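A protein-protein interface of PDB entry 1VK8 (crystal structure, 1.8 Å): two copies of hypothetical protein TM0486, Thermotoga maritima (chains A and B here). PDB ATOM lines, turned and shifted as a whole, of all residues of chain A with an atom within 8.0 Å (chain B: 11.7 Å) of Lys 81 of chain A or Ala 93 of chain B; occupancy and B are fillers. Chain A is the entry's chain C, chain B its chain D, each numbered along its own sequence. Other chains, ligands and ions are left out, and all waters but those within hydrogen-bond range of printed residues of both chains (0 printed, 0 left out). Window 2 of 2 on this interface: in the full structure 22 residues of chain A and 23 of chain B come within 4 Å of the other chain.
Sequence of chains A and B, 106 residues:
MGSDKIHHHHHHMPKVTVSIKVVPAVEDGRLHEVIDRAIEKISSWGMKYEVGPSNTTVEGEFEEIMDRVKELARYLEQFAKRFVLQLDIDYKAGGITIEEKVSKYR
The side-chain carboxylate of Glu 77 of chain A lies close to the side-chain hydroxyl of Tyr 91 of chain B (3.3 Å).
The backbone carbonyl oxygen (O) of Lys 81 of chain A is in hydrogen-bond range of the backbone NH (N) of Ala 93 of chain B (2.8 Å).
The side-chain carboxylate (OD1) of Asp 90 of chain B is in salt-bridge range of the guanidinium group (NE) of Arg 82 of chain A, 2.8 Å away.
The backbone carbonyl oxygen of Phe 83 of chain A is in hydrogen-bond range of the backbone NH of Tyr 91 of chain B (2.9 Å).
N of Ala 25 of chain A sits at hydrogen-bond distance from O of Arg 82 of chain A.
The backbone carbonyl oxygen (O) of Glu 77 of chain A is in hydrogen-bond range of the side-chain amino group (NZ) of Lys 81 of chain A (2.7 Å).
O of Gln 78 of chain A lies within hydrogen-bond range of NZ of Lys 81 of chain A, at 3.4 Å.
The backbone carbonyl oxygen (O) of Lys 15 of chain B lies within hydrogen-bond range of the backbone NH (N) of Ile 96 of chain B (2.8 Å).
O of Thr 17 of chain B sits at hydrogen-bond distance from N of Asp 90 of chain B (2.9 Å).
The side-chain amino group (NZ) of Lys 101 of chain B lies within salt-bridge range of the side-chain carboxylate (OD2) of Asp 90 of chain B, at 2.7 Å.
Among the printed residues, pairs that only touch across the chains: Arg 82 of chain A with Tyr 91 of chain B, Lys 81 of chain A with Lys 92 of chain B, Arg 82 of chain A with Lys 92 of chain B, Phe 83 of chain A with Ile 89 of chain B, Arg 82 of chain A with Ile 96 of chain B, Phe 83 of chain A with Asp 90 of chain B and Lys 81 of chain A with Tyr 91 of chain B.
No residue of chain B comes within 4 Å of Ala 25 of chain A.
Of chain B, only Tyr 91 (3.2 Å) comes within 4 Å of Glu 77 of chain A.
Gln 78 of chain A touches none of the printed residues of chain B.
Ala 80 of chain A touches none of the printed residues of chain B.
Lys 81 of chain A touches just these residues of chain B: Tyr 91, Lys 92 and Ala 93.
Printed residues of chain B within 4 Å of Arg 82 of chain A: Asp 90, Tyr 91, Lys 92 and Ile 96.
Of chain B, only Ile 89, Asp 90 and Tyr 91 come within 4 Å of Phe 83 of chain A.
Printed residues of chain A within 4 Å of Ile 89 of chain B: Phe 83 (3.9 Å).
Of the printed residues of chain A, Asp 90 of chain B touches Arg 82 (2.8 Å) and Phe 83 (3.95 Å).
Of the printed residues of chain A, Lys 92 of chain B touches Lys 81 (3.4 Å) and Arg 82 (3.5 Å).
Of chain A, only Lys 81 comes within 4 Å of Ala 93 of chain B.
Printed residues of chain A within 4 Å of Ile 96 of chain B: Arg 82.
The nearest printed residue of chain A that does not touch Tyr 91 of chain B is Ala 80 of chain A (5.7 Å).
Printed residues of chain B that touch a printed residue of chain A: Ile 89, Asp 90, Tyr 91, Lys 92, Ala 93 and Ile 96.
Hydrophobic or aromatic side chains of chain A that line the printed part of chain B: Phe 83.
Along chain A the printed residues that touch a printed residue of chain B span positions 77 to 83.
No position is printed for both chains.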
ATOM      1  N   PRO A  24     -28.866   4.594  -3.395  1.00  0.00           N
ATOM      2  CA  PRO A  24     -27.917   4.028  -4.355  1.00  0.00           C
ATOM      3  C   PRO A  24     -27.116   5.057  -5.125  1.00  0.00           C
ATOM      4  O   PRO A  24     -27.622   6.115  -5.456  1.00  0.00           O
ATOM      5  CB  PRO A  24     -28.823   3.250  -5.324  1.00  0.00           C
ATOM      6  CG  PRO A  24     -30.102   3.909  -5.239  1.00  0.00           C
ATOM      7  CD  PRO A  24     -30.241   4.541  -3.913  1.00  0.00           C
ATOM      8  N   ALA A  25     -25.873   4.722  -5.427  1.00  0.00           N
ATOM      9  CA  ALA A  25     -25.006   5.603  -6.212  1.00  0.00           C
ATOM     10  C   ALA A  25     -25.236   5.243  -7.656  1.00  0.00           C
ATOM     11  O   ALA A  25     -24.451   4.547  -8.264  1.00  0.00           O
ATOM     12  CB  ALA A  25     -23.519   5.445  -5.818  1.00  0.00           C
ATOM     13  N   VAL A  26     -26.382   5.695  -8.160  1.00  0.00           N
ATOM     14  CA  VAL A  26     -26.772   5.545  -9.541  1.00  0.00           C
ATOM     15  C   VAL A  26     -27.362   6.886  -9.993  1.00  0.00           C
ATOM     16  O   VAL A  26     -27.801   7.710  -9.166  1.00  0.00           O
ATOM     17  CB  VAL A  26     -27.796   4.378  -9.717  1.00  0.00           C
ATOM     18  CG1 VAL A  26     -27.185   3.045  -9.266  1.00  0.00           C
ATOM     19  CG2 VAL A  26     -29.090   4.644  -8.949  1.00  0.00           C
ATOM     20  N   ARG A  30     -32.444   6.078 -12.516  1.00  0.00           N
ATOM     21  CA  ARG A  30     -32.487   4.690 -12.045  1.00  0.00           C
ATOM     22  C   ARG A  30     -32.676   4.536 -10.517  1.00  0.00           C
ATOM     23  O   ARG A  30     -32.820   3.427 -10.016  1.00  0.00           O
ATOM     24  CB  ARG A  30     -31.244   3.925 -12.515  1.00  0.00           C
ATOM     25  CG  ARG A  30     -31.579   2.649 -13.313  1.00  0.00           C
ATOM     26  CD  ARG A  30     -30.453   1.644 -13.353  1.00  0.00           C
ATOM     27  NE  ARG A  30     -30.879   0.303 -12.947  1.00  0.00           N
ATOM     28  CZ  ARG A  30     -30.185  -0.497 -12.135  1.00  0.00           C
ATOM     29  NH1 ARG A  30     -29.020  -0.111 -11.630  1.00  0.00           N
ATOM     30  NH2 ARG A  30     -30.653  -1.699 -11.824  1.00  0.00           N
ATOM     31  N   VAL A  34     -33.893   0.395  -7.858  1.00  0.00           N
ATOM     32  CA  VAL A  34     -33.206  -0.082  -6.661  1.00  0.00           C
ATOM     33  C   VAL A  34     -34.114   0.022  -5.423  1.00  0.00           C
ATOM     34  O   VAL A  34     -34.208  -0.914  -4.641  1.00  0.00           O
ATOM     35  CB  VAL A  34     -31.940   0.734  -6.376  1.00  0.00           C
ATOM     36  CG1 VAL A  34     -31.242   0.213  -5.132  1.00  0.00           C
ATOM     37  CG2 VAL A  34     -31.003   0.755  -7.596  1.00  0.00           C
ATOM     38  N   TYR A  75     -28.650  -8.784  -1.378  1.00  0.00           N
ATOM     39  CA  TYR A  75     -29.638  -8.789  -2.444  1.00  0.00           C
ATOM     40  C   TYR A  75     -29.482  -7.548  -3.321  1.00  0.00           C
ATOM     41  O   TYR A  75     -29.523  -7.635  -4.548  1.00  0.00           O
ATOM     42  CB  TYR A  75     -31.040  -8.829  -1.822  1.00  0.00           C
ATOM     43  CG  TYR A  75     -32.151  -8.722  -2.813  1.00  0.00           C
ATOM     44  CD1 TYR A  75     -32.383  -9.738  -3.739  1.00  0.00           C
ATOM     45  CD2 TYR A  75     -32.986  -7.616  -2.829  1.00  0.00           C
ATOM     46  CE1 TYR A  75     -33.399  -9.636  -4.648  1.00  0.00           C
ATOM     47  CE2 TYR A  75     -34.011  -7.523  -3.725  1.00  0.00           C
ATOM     48  CZ  TYR A  75     -34.205  -8.529  -4.636  1.00  0.00           C
ATOM     49  OH  TYR A  75     -35.224  -8.416  -5.531  1.00  0.00           O
ATOM     50  N   LEU A  76     -29.309  -6.400  -2.678  1.00  0.00           N
ATOM     51  CA  LEU A  76     -29.233  -5.114  -3.374  1.00  0.00           C
ATOM     52  C   LEU A  76     -27.981  -4.929  -4.213  1.00  0.00           C
ATOM     53  O   LEU A  76     -28.008  -4.191  -5.197  1.00  0.00           O
ATOM     54  CB  LEU A  76     -29.343  -3.946  -2.403  1.00  0.00           C
ATOM     55  CG  LEU A  76     -30.725  -3.818  -1.729  1.00  0.00           C
ATOM     56  CD1 LEU A  76     -30.686  -2.700  -0.721  1.00  0.00           C
ATOM     57  CD2 LEU A  76     -31.804  -3.637  -2.779  1.00  0.00           C
ATOM     58  N   GLU A  77     -26.890  -5.592  -3.863  1.00  0.00           N
ATOM     59  CA  GLU A  77     -25.680  -5.433  -4.668  1.00  0.00           C
ATOM     60  C   GLU A  77     -25.830  -5.894  -6.113  1.00  0.00           C
ATOM     61  O   GLU A  77     -25.057  -5.463  -6.940  1.00  0.00           O
ATOM     62  CB  GLU A  77     -24.415  -6.036  -4.040  1.00  0.00           C
ATOM     63  CG  GLU A  77     -24.513  -7.400  -3.416  1.00  0.00           C
ATOM     64  CD  GLU A  77     -23.147  -7.983  -3.068  1.00  0.00           C
ATOM     65  OE1 GLU A  77     -22.124  -7.268  -3.202  1.00  0.00           O
ATOM     66  OE2 GLU A  77     -23.104  -9.172  -2.669  1.00  0.00           O
ATOM     67  N   GLN A  78     -26.816  -6.730  -6.420  1.00  0.00           N
ATOM     68  CA  GLN A  78     -27.145  -7.058  -7.818  1.00  0.00           C
ATOM     69  C   GLN A  78     -27.585  -5.819  -8.606  1.00  0.00           C
ATOM     70  O   GLN A  78     -27.428  -5.763  -9.808  1.00  0.00           O
ATOM     71  CB  GLN A  78     -28.333  -8.011  -7.938  1.00  0.00           C
ATOM     72  CG  GLN A  78     -28.414  -9.212  -7.027  1.00  0.00           C
ATOM     73  CD  GLN A  78     -29.827  -9.838  -7.031  1.00  0.00           C
ATOM     74  OE1 GLN A  78     -30.570  -9.729  -8.017  1.00  0.00           O
ATOM     75  NE2 GLN A  78     -30.183 -10.493  -5.939  1.00  0.00           N
ATOM     76  N   PHE A  79     -28.234  -4.881  -7.935  1.00  0.00           N
ATOM     77  CA  PHE A  79     -28.869  -3.727  -8.579  1.00  0.00           C
ATOM     78  C   PHE A  79     -28.045  -2.432  -8.513  1.00  0.00           C
ATOM     79  O   PHE A  79     -28.253  -1.491  -9.308  1.00  0.00           O
ATOM     80  CB  PHE A  79     -30.233  -3.509  -7.956  1.00  0.00           C
ATOM     81  CG  PHE A  79     -31.085  -4.744  -7.942  1.00  0.00           C
ATOM     82  CD1 PHE A  79     -31.447  -5.358  -9.138  1.00  0.00           C
ATOM     83  CD2 PHE A  79     -31.512  -5.305  -6.737  1.00  0.00           C
ATOM     84  CE1 PHE A  79     -32.221  -6.506  -9.135  1.00  0.00           C
ATOM     85  CE2 PHE A  79     -32.279  -6.434  -6.721  1.00  0.00           C
ATOM     86  CZ  PHE A  79     -32.645  -7.049  -7.923  1.00  0.00           C
ATOM     87  N   ALA A  80     -27.092  -2.401  -7.586  1.00  0.00           N
ATOM     88  CA  ALA A  80     -26.277  -1.227  -7.364  1.00  0.00           C
ATOM     89  C   ALA A  80     -24.982  -1.680  -6.710  1.00  0.00           C
ATOM     90  O   ALA A  80     -24.991  -2.290  -5.656  1.00  0.00           O
ATOM     91  CB  ALA A  80     -26.996  -0.257  -6.485  1.00  0.00           C
ATOM     92  N   LYS A  81     -23.890  -1.362  -7.360  1.00  0.00           N
ATOM     93  CA  LYS A  81     -22.564  -1.734  -6.908  1.00  0.00           C
ATOM     94  C   LYS A  81     -22.149  -0.900  -5.699  1.00  0.00           C
ATOM     95  O   LYS A  81     -21.236  -1.286  -4.995  1.00  0.00           O
ATOM     96  CB  LYS A  81     -21.547  -1.492  -8.022  1.00  0.00           C
ATOM     97  CG  LYS A  81     -21.273  -2.701  -8.931  1.00  0.00           C
ATOM     98  CD  LYS A  81     -22.549  -3.304  -9.492  1.00  0.00           C
ATOM     99  CE  LYS A  81     -22.914  -4.618  -8.814  1.00  0.00           C
ATOM    100  NZ  LYS A  81     -24.136  -5.228  -9.450  1.00  0.00           N
ATOM    101  N   ARG A  82     -22.769   0.261  -5.519  1.00  0.00           N
ATOM    102  CA  ARG A  82     -22.484   1.124  -4.384  1.00  0.00           C
ATOM    103  C   ARG A  82     -23.765   1.777  -3.883  1.00  0.00           C
ATOM    104  O   ARG A  82     -24.521   2.344  -4.660  1.00  0.00           O
ATOM    105  CB  ARG A  82     -21.505   2.204  -4.792  1.00  0.00           C
ATOM    106  CG  ARG A  82     -21.153   3.220  -3.720  1.00  0.00           C
ATOM    107  CD  ARG A  82     -19.905   2.879  -3.004  1.00  0.00           C
ATOM    108  NE  ARG A  82     -19.414   3.847  -2.031  1.00  0.00           N
ATOM    109  CZ  ARG A  82     -18.360   4.645  -2.194  1.00  0.00           C
ATOM    110  NH1 ARG A  82     -17.709   4.724  -3.336  1.00  0.00           N
ATOM    111  NH2 ARG A  82     -17.962   5.395  -1.193  1.00  0.00           N
ATOM    112  N   PHE A  83     -23.996   1.695  -2.584  1.00  0.00           N
ATOM    113  CA  PHE A  83     -25.152   2.318  -1.974  1.00  0.00           C
ATOM    114  C   PHE A  83     -24.905   2.613  -0.524  1.00  0.00           C
ATOM    115  O   PHE A  83     -24.091   1.954   0.129  1.00  0.00           O
ATOM    116  CB  PHE A  83     -26.437   1.476  -2.123  1.00  0.00           C
ATOM    117  CG  PHE A  83     -26.335   0.084  -1.598  1.00  0.00           C
ATOM    118  CD1 PHE A  83     -25.914  -0.951  -2.415  1.00  0.00           C
ATOM    119  CD2 PHE A  83     -26.689  -0.209  -0.294  1.00  0.00           C
ATOM    120  CE1 PHE A  83     -25.845  -2.255  -1.929  1.00  0.00           C
ATOM    121  CE2 PHE A  83     -26.584  -1.485   0.208  1.00  0.00           C
ATOM    122  CZ  PHE A  83     -26.184  -2.522  -0.613  1.00  0.00           C
ATOM    123  N   PRO B  14     -13.754  -8.032   0.946  1.00  0.00           N
ATOM    124  CA  PRO B  14     -14.364  -6.661   0.883  1.00  0.00           C
ATOM    125  C   PRO B  14     -14.897  -6.190   2.228  1.00  0.00           C
ATOM    126  O   PRO B  14     -15.655  -6.885   2.912  1.00  0.00           O
ATOM    127  CB  PRO B  14     -15.513  -6.830  -0.093  1.00  0.00           C
ATOM    128  CG  PRO B  14     -15.737  -8.320  -0.176  1.00  0.00           C
ATOM    129  CD  PRO B  14     -14.380  -8.948  -0.018  1.00  0.00           C
ATOM    130  N   LYS B  15     -14.522  -4.968   2.568  1.00  0.00           N
ATOM    131  CA  LYS B  15     -15.009  -4.308   3.752  1.00  0.00           C
ATOM    132  C   LYS B  15     -16.055  -3.266   3.437  1.00  0.00           C
ATOM    133  O   LYS B  15     -16.197  -2.802   2.312  1.00  0.00           O
ATOM    134  CB  LYS B  15     -13.839  -3.637   4.456  1.00  0.00           C
ATOM    135  CG  LYS B  15     -12.867  -4.622   5.049  1.00  0.00           C
ATOM    136  CD  LYS B  15     -11.484  -4.014   5.233  1.00  0.00           C
ATOM    137  CE  LYS B  15     -10.415  -5.116   5.451  1.00  0.00           C
ATOM    138  NZ  LYS B  15     -10.635  -6.393   4.652  1.00  0.00           N
ATOM    139  N   VAL B  16     -16.769  -2.873   4.479  1.00  0.00           N
ATOM    140  CA  VAL B  16     -17.676  -1.734   4.450  1.00  0.00           C
ATOM    141  C   VAL B  16     -17.250  -0.795   5.576  1.00  0.00           C
ATOM    142  O   VAL B  16     -16.481  -1.171   6.494  1.00  0.00           O
ATOM    143  CB  VAL B  16     -19.179  -2.143   4.679  1.00  0.00           C
ATOM    144  CG1 VAL B  16     -19.698  -3.015   3.568  1.00  0.00           C
ATOM    145  CG2 VAL B  16     -19.367  -2.889   6.024  1.00  0.00           C
ATOM    146  N   THR B  17     -17.743   0.424   5.523  1.00  0.00           N
ATOM    147  CA  THR B  17     -17.714   1.249   6.722  1.00  0.00           C
ATOM    148  C   THR B  17     -19.109   1.370   7.299  1.00  0.00           C
ATOM    149  O   THR B  17     -20.065   1.475   6.557  1.00  0.00           O
ATOM    150  CB  THR B  17     -17.119   2.663   6.446  1.00  0.00           C
ATOM    151  OG1 THR B  17     -17.991   3.412   5.602  1.00  0.00           O
ATOM    152  CG2 THR B  17     -15.831   2.549   5.695  1.00  0.00           C
ATOM    153  N   GLY B  60     -14.903  -2.975   8.493  1.00  0.00           N
ATOM    154  CA  GLY B  60     -14.734  -4.420   8.556  1.00  0.00           C
ATOM    155  C   GLY B  60     -15.762  -5.169   7.748  1.00  0.00           C
ATOM    156  O   GLY B  60     -16.451  -4.587   6.916  1.00  0.00           O
ATOM    157  N   PHE B  62     -19.071  -6.916   6.632  1.00  0.00           N
ATOM    158  CA  PHE B  62     -20.424  -6.426   6.889  1.00  0.00           C
ATOM    159  C   PHE B  62     -21.205  -7.318   7.860  1.00  0.00           C
ATOM    160  O   PHE B  62     -21.765  -6.811   8.804  1.00  0.00           O
ATOM    161  CB  PHE B  62     -21.206  -6.249   5.583  1.00  0.00           C
ATOM    162  CG  PHE B  62     -22.642  -5.836   5.778  1.00  0.00           C
ATOM    163  CD1 PHE B  62     -22.964  -4.657   6.397  1.00  0.00           C
ATOM    164  CD2 PHE B  62     -23.667  -6.640   5.321  1.00  0.00           C
ATOM    165  CE1 PHE B  62     -24.318  -4.281   6.568  1.00  0.00           C
ATOM    166  CE2 PHE B  62     -24.984  -6.259   5.497  1.00  0.00           C
ATOM    167  CZ  PHE B  62     -25.298  -5.092   6.125  1.00  0.00           C
ATOM    168  N   ILE B  89     -24.255   2.860   6.719  1.00  0.00           N
ATOM    169  CA  ILE B  89     -23.399   1.851   6.112  1.00  0.00           C
ATOM    170  C   ILE B  89     -23.056   2.304   4.705  1.00  0.00           C
ATOM    171  O   ILE B  89     -23.950   2.666   3.933  1.00  0.00           O
ATOM    172  CB  ILE B  89     -24.126   0.482   6.056  1.00  0.00           C
ATOM    173  CG1 ILE B  89     -24.555   0.046   7.458  1.00  0.00           C
ATOM    174  CG2 ILE B  89     -23.251  -0.587   5.340  1.00  0.00           C
ATOM    175  CD1 ILE B  89     -25.743  -0.851   7.468  1.00  0.00           C
ATOM    176  N   ASP B  90     -21.769   2.336   4.394  1.00  0.00           N
ATOM    177  CA  ASP B  90     -21.308   2.555   3.031  1.00  0.00           C
ATOM    178  C   ASP B  90     -20.961   1.187   2.416  1.00  0.00           C
ATOM    179  O   ASP B  90     -20.005   0.545   2.800  1.00  0.00           O
ATOM    180  CB  ASP B  90     -20.113   3.486   3.018  1.00  0.00           C
ATOM    181  CG  ASP B  90     -19.751   3.959   1.623  1.00  0.00           C
ATOM    182  OD1 ASP B  90     -20.306   3.460   0.606  1.00  0.00           O
ATOM    183  OD2 ASP B  90     -18.903   4.852   1.447  1.00  0.00           O
ATOM    184  N   TYR B  91     -21.790   0.735   1.489  1.00  0.00           N
ATOM    185  CA  TYR B  91     -21.667  -0.600   0.934  1.00  0.00           C
ATOM    186  C   TYR B  91     -21.171  -0.503  -0.492  1.00  0.00           C
ATOM    187  O   TYR B  91     -21.813   0.090  -1.322  1.00  0.00           O
ATOM    188  CB  TYR B  91     -23.021  -1.300   0.995  1.00  0.00           C
ATOM    189  CG  TYR B  91     -22.960  -2.812   0.776  1.00  0.00           C
ATOM    190  CD1 TYR B  91     -22.816  -3.324  -0.496  1.00  0.00           C
ATOM    191  CD2 TYR B  91     -23.023  -3.718   1.859  1.00  0.00           C
ATOM    192  CE1 TYR B  91     -22.776  -4.712  -0.739  1.00  0.00           C
ATOM    193  CE2 TYR B  91     -22.960  -5.120   1.630  1.00  0.00           C
ATOM    194  CZ  TYR B  91     -22.843  -5.599   0.319  1.00  0.00           C
ATOM    195  OH  TYR B  91     -22.788  -6.952  -0.025  1.00  0.00           O
ATOM    196  N   LYS B  92     -19.986  -1.043  -0.759  1.00  0.00           N
ATOM    197  CA  LYS B  92     -19.427  -1.061  -2.113  1.00  0.00           C
ATOM    198  C   LYS B  92     -18.983  -2.474  -2.498  1.00  0.00           C
ATOM    199  O   LYS B  92     -18.211  -3.114  -1.786  1.00  0.00           O
ATOM    200  CB  LYS B  92     -18.222  -0.114  -2.199  1.00  0.00           C
ATOM    201  CG  LYS B  92     -17.733   0.141  -3.581  1.00  0.00           C
ATOM    202  CD  LYS B  92     -16.481   0.983  -3.567  1.00  0.00           C
ATOM    203  CE  LYS B  92     -15.880   1.140  -4.965  1.00  0.00           C
ATOM    204  NZ  LYS B  92     -14.788   2.156  -4.906  1.00  0.00           N
ATOM    205  N   ALA B  93     -19.446  -2.951  -3.645  1.00  0.00           N
ATOM    206  CA  ALA B  93     -18.977  -4.218  -4.159  1.00  0.00           C
ATOM    207  C   ALA B  93     -17.462  -4.150  -4.346  1.00  0.00           C
ATOM    208  O   ALA B  93     -16.928  -3.249  -5.017  1.00  0.00           O
ATOM    209  CB  ALA B  93     -19.673  -4.552  -5.484  1.00  0.00           C
ATOM    210  N   GLY B  94     -16.754  -5.102  -3.781  1.00  0.00           N
ATOM    211  CA  GLY B  94     -15.310  -5.099  -3.913  1.00  0.00           C
ATOM    212  C   GLY B  94     -14.632  -4.400  -2.744  1.00  0.00           C
ATOM    213  O   GLY B  94     -13.411  -4.441  -2.618  1.00  0.00           O
ATOM    214  N   GLY B  95     -15.426  -3.733  -1.913  1.00  0.00           N
ATOM    215  CA  GLY B  95     -14.982  -3.199  -0.640  1.00  0.00           C
ATOM    216  C   GLY B  95     -14.786  -1.694  -0.651  1.00  0.00           C
ATOM    217  O   GLY B  95     -14.521  -1.106  -1.699  1.00  0.00           O
ATOM    218  N   ILE B  96     -14.912  -1.077   0.526  1.00  0.00           N
ATOM    219  CA  ILE B  96     -14.594   0.342   0.734  1.00  0.00           C
ATOM    220  C   ILE B  96     -14.020   0.539   2.147  1.00  0.00           C
ATOM    221  O   ILE B  96     -14.412  -0.155   3.088  1.00  0.00           O
ATOM    222  CB  ILE B  96     -15.872   1.244   0.504  1.00  0.00           C
ATOM    223  CG1 ILE B  96     -15.545   2.742   0.555  1.00  0.00           C
ATOM    224  CG2 ILE B  96     -16.996   0.932   1.490  1.00  0.00           C
ATOM    225  CD1 ILE B  96     -14.743   3.219  -0.606  1.00  0.00           C
ATOM    226  N   THR B  97     -13.129   1.509   2.296  1.00  0.00           N
ATOM    227  CA  THR B  97     -12.412   1.732   3.544  1.00  0.00           C
ATOM    228  C   THR B  97     -12.497   3.172   4.028  1.00  0.00           C
ATOM    229  O   THR B  97     -12.779   4.084   3.262  1.00  0.00           O
ATOM    230  CB  THR B  97     -10.929   1.375   3.392  1.00  0.00           C
ATOM    231  OG1 THR B  97     -10.331   2.183   2.376  1.00  0.00           O
ATOM    232  CG2 THR B  97     -10.723  -0.056   2.938  1.00  0.00           C
ATOM    233  N   GLU B 100      -9.950   5.448   2.120  1.00  0.00           N
ATOM    234  CA  GLU B 100     -10.378   5.810   0.765  1.00  0.00           C
ATOM    235  C   GLU B 100     -11.333   6.993   0.821  1.00  0.00           C
ATOM    236  O   GLU B 100     -11.396   7.786  -0.092  1.00  0.00           O
ATOM    237  CB  GLU B 100     -11.098   4.643   0.085  1.00  0.00           C
ATOM    238  CG  GLU B 100     -10.168   3.587  -0.486  1.00  0.00           C
ATOM    239  CD  GLU B 100     -10.907   2.345  -0.934  1.00  0.00           C
ATOM    240  OE1 GLU B 100     -11.229   1.493  -0.074  1.00  0.00           O
ATOM    241  OE2 GLU B 100     -11.167   2.234  -2.149  1.00  0.00           O
ATOM    242  N   LYS B 101     -12.067   7.096   1.921  1.00  0.00           N
ATOM    243  CA  LYS B 101     -13.013   8.184   2.125  1.00  0.00           C
ATOM    244  C   LYS B 101     -12.383   9.468   2.741  1.00  0.00           C
ATOM    245  O   LYS B 101     -12.839  10.567   2.446  1.00  0.00           O
ATOM    246  CB  LYS B 101     -14.180   7.667   2.973  1.00  0.00           C
ATOM    247  CG  LYS B 101     -15.303   6.941   2.185  1.00  0.00           C
ATOM    248  CD  LYS B 101     -15.765   5.647   2.826  1.00  0.00           C
ATOM    249  CE  LYS B 101     -16.742   5.804   3.986  1.00  0.00           C
ATOM    250  NZ  LYS B 101     -18.040   6.329   3.556  1.00  0.00           N
